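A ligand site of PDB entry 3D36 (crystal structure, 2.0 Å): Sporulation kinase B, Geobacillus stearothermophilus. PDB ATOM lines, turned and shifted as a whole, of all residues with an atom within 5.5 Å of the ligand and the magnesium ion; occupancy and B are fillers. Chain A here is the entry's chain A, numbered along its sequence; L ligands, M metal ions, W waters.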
ATOM      1  N   ASP A  69     -35.716 -10.523  25.142  1.00  0.00           N
ATOM      2  CA  ASP A  69     -35.223 -10.567  26.528  1.00  0.00           C
ATOM      3  C   ASP A  69     -35.991  -9.651  27.486  1.00  0.00           C
ATOM      4  O   ASP A  69     -36.152  -9.973  28.665  1.00  0.00           O
ATOM      5  CB  ASP A  69     -33.746 -10.206  26.595  1.00  0.00           C
ATOM      6  CG  ASP A  69     -32.841 -11.304  26.080  1.00  0.00           C
ATOM      7  OD1 ASP A  69     -33.058 -12.489  26.392  1.00  0.00           O
ATOM      8  OD2 ASP A  69     -31.881 -10.957  25.359  1.00  0.00           O
ATOM      9  N   ASN A 130     -37.144 -16.334  29.747  1.00  0.00           N
ATOM     10  CA  ASN A 130     -35.694 -16.179  29.627  1.00  0.00           C
ATOM     11  C   ASN A 130     -34.930 -17.396  30.113  1.00  0.00           C
ATOM     12  O   ASN A 130     -33.956 -17.816  29.483  1.00  0.00           O
ATOM     13  CB  ASN A 130     -35.224 -14.905  30.341  1.00  0.00           C
ATOM     14  CG  ASN A 130     -35.610 -13.645  29.609  1.00  0.00           C
ATOM     15  OD1 ASN A 130     -36.342 -13.676  28.624  1.00  0.00           O
ATOM     16  ND2 ASN A 130     -35.108 -12.512  30.084  1.00  0.00           N
ATOM     17  N   VAL A 131     -35.380 -17.968  31.227  1.00  0.00           N
ATOM     18  CA  VAL A 131     -34.771 -19.191  31.782  1.00  0.00           C
ATOM     19  C   VAL A 131     -34.995 -20.387  30.858  1.00  0.00           C
ATOM     20  O   VAL A 131     -34.042 -21.107  30.522  1.00  0.00           O
ATOM     21  CB  VAL A 131     -35.317 -19.497  33.200  1.00  0.00           C
ATOM     22  CG1 VAL A 131     -34.778 -20.837  33.716  1.00  0.00           C
ATOM     23  CG2 VAL A 131     -34.953 -18.381  34.170  1.00  0.00           C
ATOM     24  N   ASN A 134     -33.160 -20.201  27.380  1.00  0.00           N
ATOM     25  CA  ASN A 134     -31.768 -20.598  27.608  1.00  0.00           C
ATOM     26  C   ASN A 134     -31.587 -22.107  27.670  1.00  0.00           C
ATOM     27  O   ASN A 134     -30.609 -22.642  27.145  1.00  0.00           O
ATOM     28  CB  ASN A 134     -31.257 -19.980  28.912  1.00  0.00           C
ATOM     29  CG  ASN A 134     -30.897 -18.525  28.777  1.00  0.00           C
ATOM     30  OD1 ASN A 134     -30.755 -18.012  27.670  1.00  0.00           O
ATOM     31  ND2 ASN A 134     -30.739 -17.859  29.904  1.00  0.00           N
ATOM     32  N   ALA A 135     -32.531 -22.794  28.316  1.00  0.00           N
ATOM     33  CA  ALA A 135     -32.475 -24.247  28.471  1.00  0.00           C
ATOM     34  C   ALA A 135     -32.619 -24.951  27.124  1.00  0.00           C
ATOM     35  O   ALA A 135     -31.923 -25.920  26.853  1.00  0.00           O
ATOM     36  CB  ALA A 135     -33.541 -24.720  29.450  1.00  0.00           C
ATOM     37  N   GLU A 137     -31.985 -23.527  24.151  1.00  0.00           N
ATOM     38  CA  GLU A 137     -30.807 -23.129  23.359  1.00  0.00           C
ATOM     39  C   GLU A 137     -29.544 -23.893  23.751  1.00  0.00           C
ATOM     40  O   GLU A 137     -28.593 -23.982  22.963  1.00  0.00           O
ATOM     41  CB  GLU A 137     -30.580 -21.623  23.453  1.00  0.00           C
ATOM     42  CG  GLU A 137     -31.605 -20.801  22.677  1.00  0.00           C
ATOM     43  CD  GLU A 137     -31.556 -19.322  22.991  1.00  0.00           C
ATOM     44  OE1 GLU A 137     -32.130 -18.536  22.210  1.00  0.00           O
ATOM     45  OE2 GLU A 137     -30.957 -18.936  24.022  1.00  0.00           O
ATOM     46  N   ALA A 138     -29.527 -24.435  24.967  1.00  0.00           N
ATOM     47  CA  ALA A 138     -28.426 -25.276  25.449  1.00  0.00           C
ATOM     48  C   ALA A 138     -28.515 -26.683  24.871  1.00  0.00           C
ATOM     49  O   ALA A 138     -27.569 -27.469  24.974  1.00  0.00           O
ATOM     50  CB  ALA A 138     -28.429 -25.326  26.968  1.00  0.00           C
ATOM     51  N   ASP A 162     -32.348 -28.937  32.204  1.00  0.00           N
ATOM     52  CA  ASP A 162     -32.049 -29.298  30.819  1.00  0.00           C
ATOM     53  C   ASP A 162     -30.884 -30.275  30.778  1.00  0.00           C
ATOM     54  O   ASP A 162     -30.067 -30.339  31.699  1.00  0.00           O
ATOM     55  CB  ASP A 162     -31.748 -28.046  29.978  1.00  0.00           C
ATOM     56  CG  ASP A 162     -30.502 -27.309  30.448  1.00  0.00           C
ATOM     57  OD1 ASP A 162     -29.389 -27.831  30.272  1.00  0.00           O
ATOM     58  OD2 ASP A 162     -30.652 -26.183  30.969  1.00  0.00           O
ATOM     59  N   VAL A 165     -25.621 -28.335  27.098  1.00  0.00           N
ATOM     60  CA  VAL A 165     -24.173 -28.166  27.084  1.00  0.00           C
ATOM     61  C   VAL A 165     -23.551 -27.898  28.453  1.00  0.00           C
ATOM     62  O   VAL A 165     -22.365 -28.166  28.668  1.00  0.00           O
ATOM     63  CB  VAL A 165     -23.705 -27.083  26.065  1.00  0.00           C
ATOM     64  CG1 VAL A 165     -23.964 -27.538  24.636  1.00  0.00           C
ATOM     65  CG2 VAL A 165     -24.380 -25.730  26.337  1.00  0.00           C
ATOM     66  N   GLY A 166     -24.346 -27.365  29.379  1.00  0.00           N
ATOM     67  CA  GLY A 166     -23.886 -27.046  30.724  1.00  0.00           C
ATOM     68  C   GLY A 166     -22.989 -25.816  30.772  1.00  0.00           C
ATOM     69  O   GLY A 166     -22.797 -25.131  29.763  1.00  0.00           O
ATOM     70  N   MET A 167     -22.459 -25.535  31.965  1.00  0.00           N
ATOM     71  CA  MET A 167     -21.539 -24.433  32.176  1.00  0.00           C
ATOM     72  C   MET A 167     -20.356 -24.858  33.042  1.00  0.00           C
ATOM     73  O   MET A 167     -20.514 -25.671  33.951  1.00  0.00           O
ATOM     74  CB  MET A 167     -22.248 -23.254  32.840  1.00  0.00           C
ATOM     75  CG  MET A 167     -23.113 -22.422  31.896  1.00  0.00           C
ATOM     76  SD  MET A 167     -24.170 -21.258  32.780  1.00  0.00           S
ATOM     77  CE  MET A 167     -25.528 -22.319  33.277  1.00  0.00           C
ATOM     78  N   LEU A 175     -22.743 -15.960  35.082  1.00  0.00           N
ATOM     79  CA  LEU A 175     -24.116 -16.038  34.595  1.00  0.00           C
ATOM     80  C   LEU A 175     -24.950 -14.902  35.186  1.00  0.00           C
ATOM     81  O   LEU A 175     -25.071 -14.773  36.409  1.00  0.00           O
ATOM     82  CB  LEU A 175     -24.731 -17.401  34.946  1.00  0.00           C
ATOM     83  CG  LEU A 175     -26.196 -17.688  34.648  1.00  0.00           C
ATOM     84  CD1 LEU A 175     -26.443 -17.745  33.157  1.00  0.00           C
ATOM     85  CD2 LEU A 175     -26.629 -18.991  35.294  1.00  0.00           C
ATOM     86  N   GLY A 176     -25.509 -14.061  34.312  1.00  0.00           N
ATOM     87  CA  GLY A 176     -26.333 -12.933  34.748  1.00  0.00           C
ATOM     88  C   GLY A 176     -25.601 -11.605  34.795  1.00  0.00           C
ATOM     89  O   GLY A 176     -26.230 -10.562  34.988  1.00  0.00           O
ATOM     90  N   PHE A 180     -22.546 -10.605  29.366  1.00  0.00           N
ATOM     91  CA  PHE A 180     -21.787 -11.857  29.314  1.00  0.00           C
ATOM     92  C   PHE A 180     -22.589 -12.898  28.553  1.00  0.00           C
ATOM     93  O   PHE A 180     -23.679 -13.287  28.972  1.00  0.00           O
ATOM     94  CB  PHE A 180     -21.389 -12.373  30.701  1.00  0.00           C
ATOM     95  CG  PHE A 180     -20.812 -13.762  30.674  1.00  0.00           C
ATOM     96  CD1 PHE A 180     -19.556 -14.004  30.129  1.00  0.00           C
ATOM     97  CD2 PHE A 180     -21.541 -14.847  31.186  1.00  0.00           C
ATOM     98  CE1 PHE A 180     -19.013 -15.297  30.090  1.00  0.00           C
ATOM     99  CE2 PHE A 180     -21.006 -16.141  31.151  1.00  0.00           C
ATOM    100  CZ  PHE A 180     -19.749 -16.364  30.614  1.00  0.00           C
ATOM    101  N   THR A 181     -22.027 -13.347  27.426  1.00  0.00           N
ATOM    102  CA  THR A 181     -22.665 -14.333  26.576  1.00  0.00           C
ATOM    103  C   THR A 181     -21.614 -15.204  25.888  1.00  0.00           C
ATOM    104  O   THR A 181     -20.496 -14.753  25.640  1.00  0.00           O
ATOM    105  CB  THR A 181     -23.598 -13.667  25.522  1.00  0.00           C
ATOM    106  OG1 THR A 181     -24.219 -14.685  24.722  1.00  0.00           O
ATOM    107  CG2 THR A 181     -22.829 -12.709  24.614  1.00  0.00           C
ATOM    108  N   THR A 182     -21.986 -16.449  25.609  1.00  0.00           N
ATOM    109  CA  THR A 182     -21.129 -17.372  24.868  1.00  0.00           C
ATOM    110  C   THR A 182     -21.728 -17.705  23.493  1.00  0.00           C
ATOM    111  O   THR A 182     -21.259 -18.618  22.808  1.00  0.00           O
ATOM    112  CB  THR A 182     -20.910 -18.698  25.638  1.00  0.00           C
ATOM    113  OG1 THR A 182     -22.187 -19.263  25.957  1.00  0.00           O
ATOM    114  CG2 THR A 182     -20.107 -18.465  26.918  1.00  0.00           C
ATOM    115  N   LYS A 183     -22.763 -16.961  23.103  1.00  0.00           N
ATOM    116  CA  LYS A 183     -23.538 -17.295  21.910  1.00  0.00           C
ATOM    117  C   LYS A 183     -23.167 -16.463  20.673  1.00  0.00           C
ATOM    118  O   LYS A 183     -23.850 -16.528  19.647  1.00  0.00           O
ATOM    119  CB  LYS A 183     -25.037 -17.197  22.205  1.00  0.00           C
ATOM    120  CG  LYS A 183     -25.532 -18.316  23.100  1.00  0.00           C
ATOM    121  CD  LYS A 183     -26.934 -18.048  23.626  1.00  0.00           C
ATOM    122  CE  LYS A 183     -27.295 -19.074  24.685  1.00  0.00           C
ATOM    123  NZ  LYS A 183     -28.572 -18.763  25.369  1.00  0.00           N
ATOM    124  N   LYS A 186     -25.565 -13.805  18.173  1.00  0.00           N
ATOM    125  CA  LYS A 186     -26.946 -14.059  18.590  1.00  0.00           C
ATOM    126  C   LYS A 186     -27.191 -13.853  20.084  1.00  0.00           C
ATOM    127  O   LYS A 186     -28.333 -13.809  20.541  1.00  0.00           O
ATOM    128  CB  LYS A 186     -27.397 -15.464  18.161  1.00  0.00           C
ATOM    129  CG  LYS A 186     -27.572 -15.627  16.644  1.00  0.00           C
ATOM    130  CD  LYS A 186     -28.530 -16.767  16.290  1.00  0.00           C
ATOM    131  CE  LYS A 186     -27.837 -18.124  16.338  1.00  0.00           C
ATOM    132  NZ  LYS A 186     -28.778 -19.239  15.998  1.00  0.00           N
ATOM    133  N   GLY A 187     -26.106 -13.722  20.849  1.00  0.00           N
ATOM    134  CA  GLY A 187     -26.186 -13.518  22.290  1.00  0.00           C
ATOM    135  C   GLY A 187     -26.330 -12.056  22.688  1.00  0.00           C
ATOM    136  O   GLY A 187     -25.849 -11.176  21.976  1.00  0.00           O
ATOM    137  N   THR A 188     -27.006 -11.816  23.809  1.00  0.00           N
ATOM    138  CA  THR A 188     -27.106 -10.487  24.405  1.00  0.00           C
ATOM    139  C   THR A 188     -26.441 -10.445  25.786  1.00  0.00           C
ATOM    140  O   THR A 188     -25.853  -9.430  26.174  1.00  0.00           O
ATOM    141  CB  THR A 188     -28.577 -10.025  24.579  1.00  0.00           C
ATOM    142  OG1 THR A 188     -29.251 -10.865  25.511  1.00  0.00           O
ATOM    143  CG2 THR A 188     -29.314 -10.050  23.233  1.00  0.00           C
ATOM    144  N   GLY A 189     -26.539 -11.540  26.537  1.00  0.00           N
ATOM    145  CA  GLY A 189     -26.044 -11.590  27.907  1.00  0.00           C
ATOM    146  C   GLY A 189     -26.883 -10.752  28.870  1.00  0.00           C
ATOM    147  O   GLY A 189     -26.393 -10.335  29.913  1.00  0.00           O
ATOM    148  N   LEU A 190     -28.138 -10.513  28.497  1.00  0.00           N
ATOM    149  CA  LEU A 190     -29.038  -9.664  29.277  1.00  0.00           C
ATOM    150  C   LEU A 190     -30.283 -10.405  29.770  1.00  0.00           C
ATOM    151  O   LEU A 190     -31.046  -9.874  30.604  1.00  0.00           O
ATOM    152  CB  LEU A 190     -29.446  -8.433  28.458  1.00  0.00           C
ATOM    153  CG  LEU A 190     -28.304  -7.486  28.052  1.00  0.00           C
ATOM    154  CD1 LEU A 190     -28.713  -6.567  26.887  1.00  0.00           C
ATOM    155  CD2 LEU A 190     -27.806  -6.663  29.246  1.00  0.00           C
ATOM    156  N   GLY A 191     -30.490 -11.621  29.268  1.00  0.00           N
ATOM    157  CA  GLY A 191     -31.658 -12.426  29.618  1.00  0.00           C
ATOM    158  C   GLY A 191     -31.669 -12.880  31.071  1.00  0.00           C
ATOM    159  O   GLY A 191     -32.670 -12.720  31.771  1.00  0.00           O
ATOM    160  N   MET A 192     -30.556 -13.443  31.524  1.00  0.00           N
ATOM    161  CA  MET A 192     -30.476 -13.898  32.915  1.00  0.00           C
ATOM    162  C   MET A 192     -30.435 -12.750  33.917  1.00  0.00           C
ATOM    163  O   MET A 192     -30.959 -12.870  35.027  1.00  0.00           O
ATOM    164  CB  MET A 192     -29.306 -14.851  33.127  1.00  0.00           C
ATOM    165  CG  MET A 192     -29.685 -16.312  32.939  1.00  0.00           C
ATOM    166  SD  MET A 192     -31.048 -16.856  34.012  1.00  0.00           S
ATOM    167  CE  MET A 192     -30.479 -16.355  35.611  1.00  0.00           C
ATOM    168  N   MET A 193     -29.824 -11.642  33.528  1.00  0.00           N
ATOM    169  CA  MET A 193     -29.779 -10.427  34.349  1.00  0.00           C
ATOM    170  C   MET A 193     -31.176  -9.962  34.776  1.00  0.00           C
ATOM    171  O   MET A 193     -31.404  -9.599  35.929  1.00  0.00           O
ATOM    172  CB  MET A 193     -29.080  -9.310  33.587  1.00  0.00           C
ATOM    173  CG  MET A 193     -28.994  -7.991  34.346  1.00  0.00           C
ATOM    174  SD  MET A 193     -28.619  -6.596  33.272  1.00  0.00           S
ATOM    175  CE  MET A 193     -30.137  -6.468  32.309  1.00  0.00           C
ATOM    176  N   THR A 216     -28.058 -28.307  33.039  1.00  0.00           N
ATOM    177  CA  THR A 216     -28.235 -27.188  33.963  1.00  0.00           C
ATOM    178  C   THR A 216     -29.604 -27.241  34.645  1.00  0.00           C
ATOM    179  O   THR A 216     -30.621 -27.450  33.980  1.00  0.00           O
ATOM    180  CB  THR A 216     -28.095 -25.841  33.215  1.00  0.00           C
ATOM    181  OG1 THR A 216     -26.829 -25.791  32.550  1.00  0.00           O
ATOM    182  CG2 THR A 216     -28.209 -24.659  34.181  1.00  0.00           C
HETATM  183  P1  LIG L   1     -27.813 -15.054  26.143  1.00  0.00           P
HETATM  184  O1  LIG L   1     -26.392 -15.493  25.897  1.00  0.00           O
HETATM  185  O2  LIG L   1     -28.786 -16.195  26.285  1.00  0.00           O
HETATM  186  O3  LIG L   1     -28.282 -13.990  25.185  1.00  0.00           O
HETATM  187  P2  LIG L   1     -28.305 -14.841  28.972  1.00  0.00           P
HETATM  188  O4  LIG L   1     -29.665 -15.460  28.775  1.00  0.00           O
HETATM  189  O5  LIG L   1     -28.137 -13.722  29.977  1.00  0.00           O
HETATM  190  O6  LIG L   1     -27.753 -14.286  27.551  1.00  0.00           O
HETATM  191  O7  LIG L   1     -27.274 -16.017  29.368  1.00  0.00           O
HETATM  192  C1  LIG L   1     -25.883 -15.715  29.480  1.00  0.00           C
HETATM  193  C2  LIG L   1     -25.017 -16.945  29.244  1.00  0.00           C
HETATM  194  O8  LIG L   1     -25.183 -17.886  30.297  1.00  0.00           O
HETATM  195  C3  LIG L   1     -25.345 -17.707  27.972  1.00  0.00           C
HETATM  196  O9  LIG L   1     -24.668 -17.157  26.836  1.00  0.00           O
HETATM  197  C4  LIG L   1     -24.870 -19.104  28.291  1.00  0.00           C
HETATM  198  O10 LIG L   1     -23.479 -19.242  27.999  1.00  0.00           O
HETATM  199  C5  LIG L   1     -25.061 -19.217  29.786  1.00  0.00           C
HETATM  200  N1  LIG L   1     -26.280 -20.016  30.080  1.00  0.00           N
HETATM  201  C6  LIG L   1     -27.453 -19.534  30.528  1.00  0.00           C
HETATM  202  N2  LIG L   1     -28.363 -20.525  30.679  1.00  0.00           N
HETATM  203  C7  LIG L   1     -27.777 -21.675  30.326  1.00  0.00           C
HETATM  204  C8  LIG L   1     -28.169 -23.099  30.247  1.00  0.00           C
HETATM  205  N3  LIG L   1     -29.416 -23.498  30.601  1.00  0.00           N
HETATM  206  N4  LIG L   1     -27.242 -23.998  29.821  1.00  0.00           N
HETATM  207  C9  LIG L   1     -25.997 -23.618  29.460  1.00  0.00           C
HETATM  208  N5  LIG L   1     -25.568 -22.336  29.505  1.00  0.00           N
HETATM  209  C10 LIG L   1     -26.395 -21.339  29.920  1.00  0.00           C
HETATM  210 MG    MG M   1     -30.675 -15.957  26.977  1.00  0.00          MG
HETATM  211  O   HOH W   1     -31.941 -22.316  31.898  1.00  0.00           O
HETATM  212  O   HOH W   2     -30.840 -13.889  26.508  1.00  0.00           O
HETATM  213  O   HOH W   3     -27.736 -11.851  31.654  1.00  0.00           O
HETATM  214  O   HOH W   4     -30.747 -19.936  32.332  1.00  0.00           O
HETATM  215  O   HOH W   5     -29.738 -14.079  23.028  1.00  0.00           O
HETATM  216  O   HOH W   6     -24.873 -13.183  31.475  1.00  0.00           O
HETATM  217  O   HOH W   7     -27.107 -26.679  30.070  1.00  0.00           O
HETATM  218  O   HOH W   8     -32.678 -15.785  28.116  1.00  0.00           O
HETATM  219  O   HOH W   9     -31.663 -16.603  25.137  1.00  0.00           O
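The backbone NH (N) of Thr 182 is in hydrogen-bond range of an oxygen (O9) of the ligand. OG1 of Thr 182 lies within hydrogen-bond range of O10 of the ligand (2.4 Å). The side-chain hydroxyl of Thr 181 lies within hydrogen-bond range of an oxygen (O1) of the ligand, 2.6 Å away. An oxygen (O1) of the ligand lies within salt-bridge range of the side-chain amino group of Lys 183 (3.97 Å). O3 of the ligand sits at hydrogen-bond distance from N of Thr 188 (2.9 Å). The side-chain hydroxyl (OG1) of Thr 188 is in hydrogen-bond range of an oxygen (O3) of the ligand, 3.3 Å away. An oxygen (O5) of the ligand is in hydrogen-bond range of the backbone NH (N) of Met 192, 2.9 Å away. The side-chain carboxylate of Asp 162 sits at hydrogen-bond distance from a nitrogen (N3) of the ligand (3.0 Å). An oxygen (O6) of the ligand is in hydrogen-bond range of the backbone NH (N) of Gly 189, 3.2 Å away. An oxygen (O5) of the ligand lies within hydrogen-bond range of the backbone NH (N) of Gly 191, at 3.2 Å. OG1 of Thr 216 is in hydrogen-bond range of N4 of the ligand (3.3 Å).
OD1 of Asn 134 lies close to NZ of Lys 183, 3.3 Å away. ND2 of Asn 134 lies close to O of Asn 130, 3.2 Å away. The side-chain hydroxyl of Thr 181 lies within hydrogen-bond range of the backbone NH of Lys 183 (3.1 Å). The side-chain carboxylate (OE2) of Glu 137 lies within salt-bridge range of the side-chain amino group (NZ) of Lys 183. The backbone NH (N) of Leu 190 lies close to the side-chain hydroxyl (OG1) of Thr 188. The side-chain hydroxyl of Thr 188 is in hydrogen-bond range of the side-chain carboxylate of Asp 69. O of Gly 191 lies within hydrogen-bond range of ND2 of Asn 130 (3.0 Å). O of Ala 138 sits at hydrogen-bond distance from N of Val 165, 3.0 Å away.
The side-chain sulfur (SD) of Met 167 sits close to a nitrogen (N1) of the ligand (3.6 Å). CA of Ala 135 touches N3 of the ligand, 3.8 Å away. Ala 138 touches the ligand (CB to N4, 3.4 Å). Gly 166 touches the ligand (O to C9, 3.6 Å). Leu 175 touches the ligand (CD1 to O8, 3.1 Å). Phe 180 touches the ligand. CA of Gly 187 touches O3 of the ligand, at 3.6 Å. N of Leu 190 touches O5 of the ligand (3.5 Å). Of the 26 residues printed, 18 come within 4 Å of the ligand. The nearest printed residue that does not touch the ligand is Val 165 (4.1 Å).
Merely in contact with the magnesium ion: Lys 183. Of the 26 residues printed, 2 come within 4 Å of the magnesium ion.
The magnesium ion is bound by an oxygen (O2) of the ligand, an oxygen (O4) of the ligand, water W2, the side-chain amide oxygen of Asn 134, water W9 and water W8.
Water W2 bridges OD1 of Asp 69 (2.6 Å) and O3 of the ligand (2.9 Å). Water W8 lies within hydrogen-bond range of O of Asn 130 (2.8 Å) and ND2 of Asn 134 (3.4 Å). Water W5 bridges O3 of the ligand (2.6 Å) and O of Lys 186 (2.9 Å). Water W7 lies within hydrogen-bond range of OD1 of Asp 162 (2.6 Å), OG1 of Thr 216 (2.6 Å), N4 of the ligand (2.7 Å) and N of Gly 166 (2.9 Å). Water W4 lies within hydrogen-bond range of a nitrogen (N2) of the ligand (3.0 Å), the side-chain amide nitrogen of Asn 134 (3.2 Å) and the side-chain sulfur of Met 192 (3.5 Å). Water W1 lies within hydrogen-bond range of the backbone carbonyl oxygen of Val 131 and a nitrogen (N3) of the ligand.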
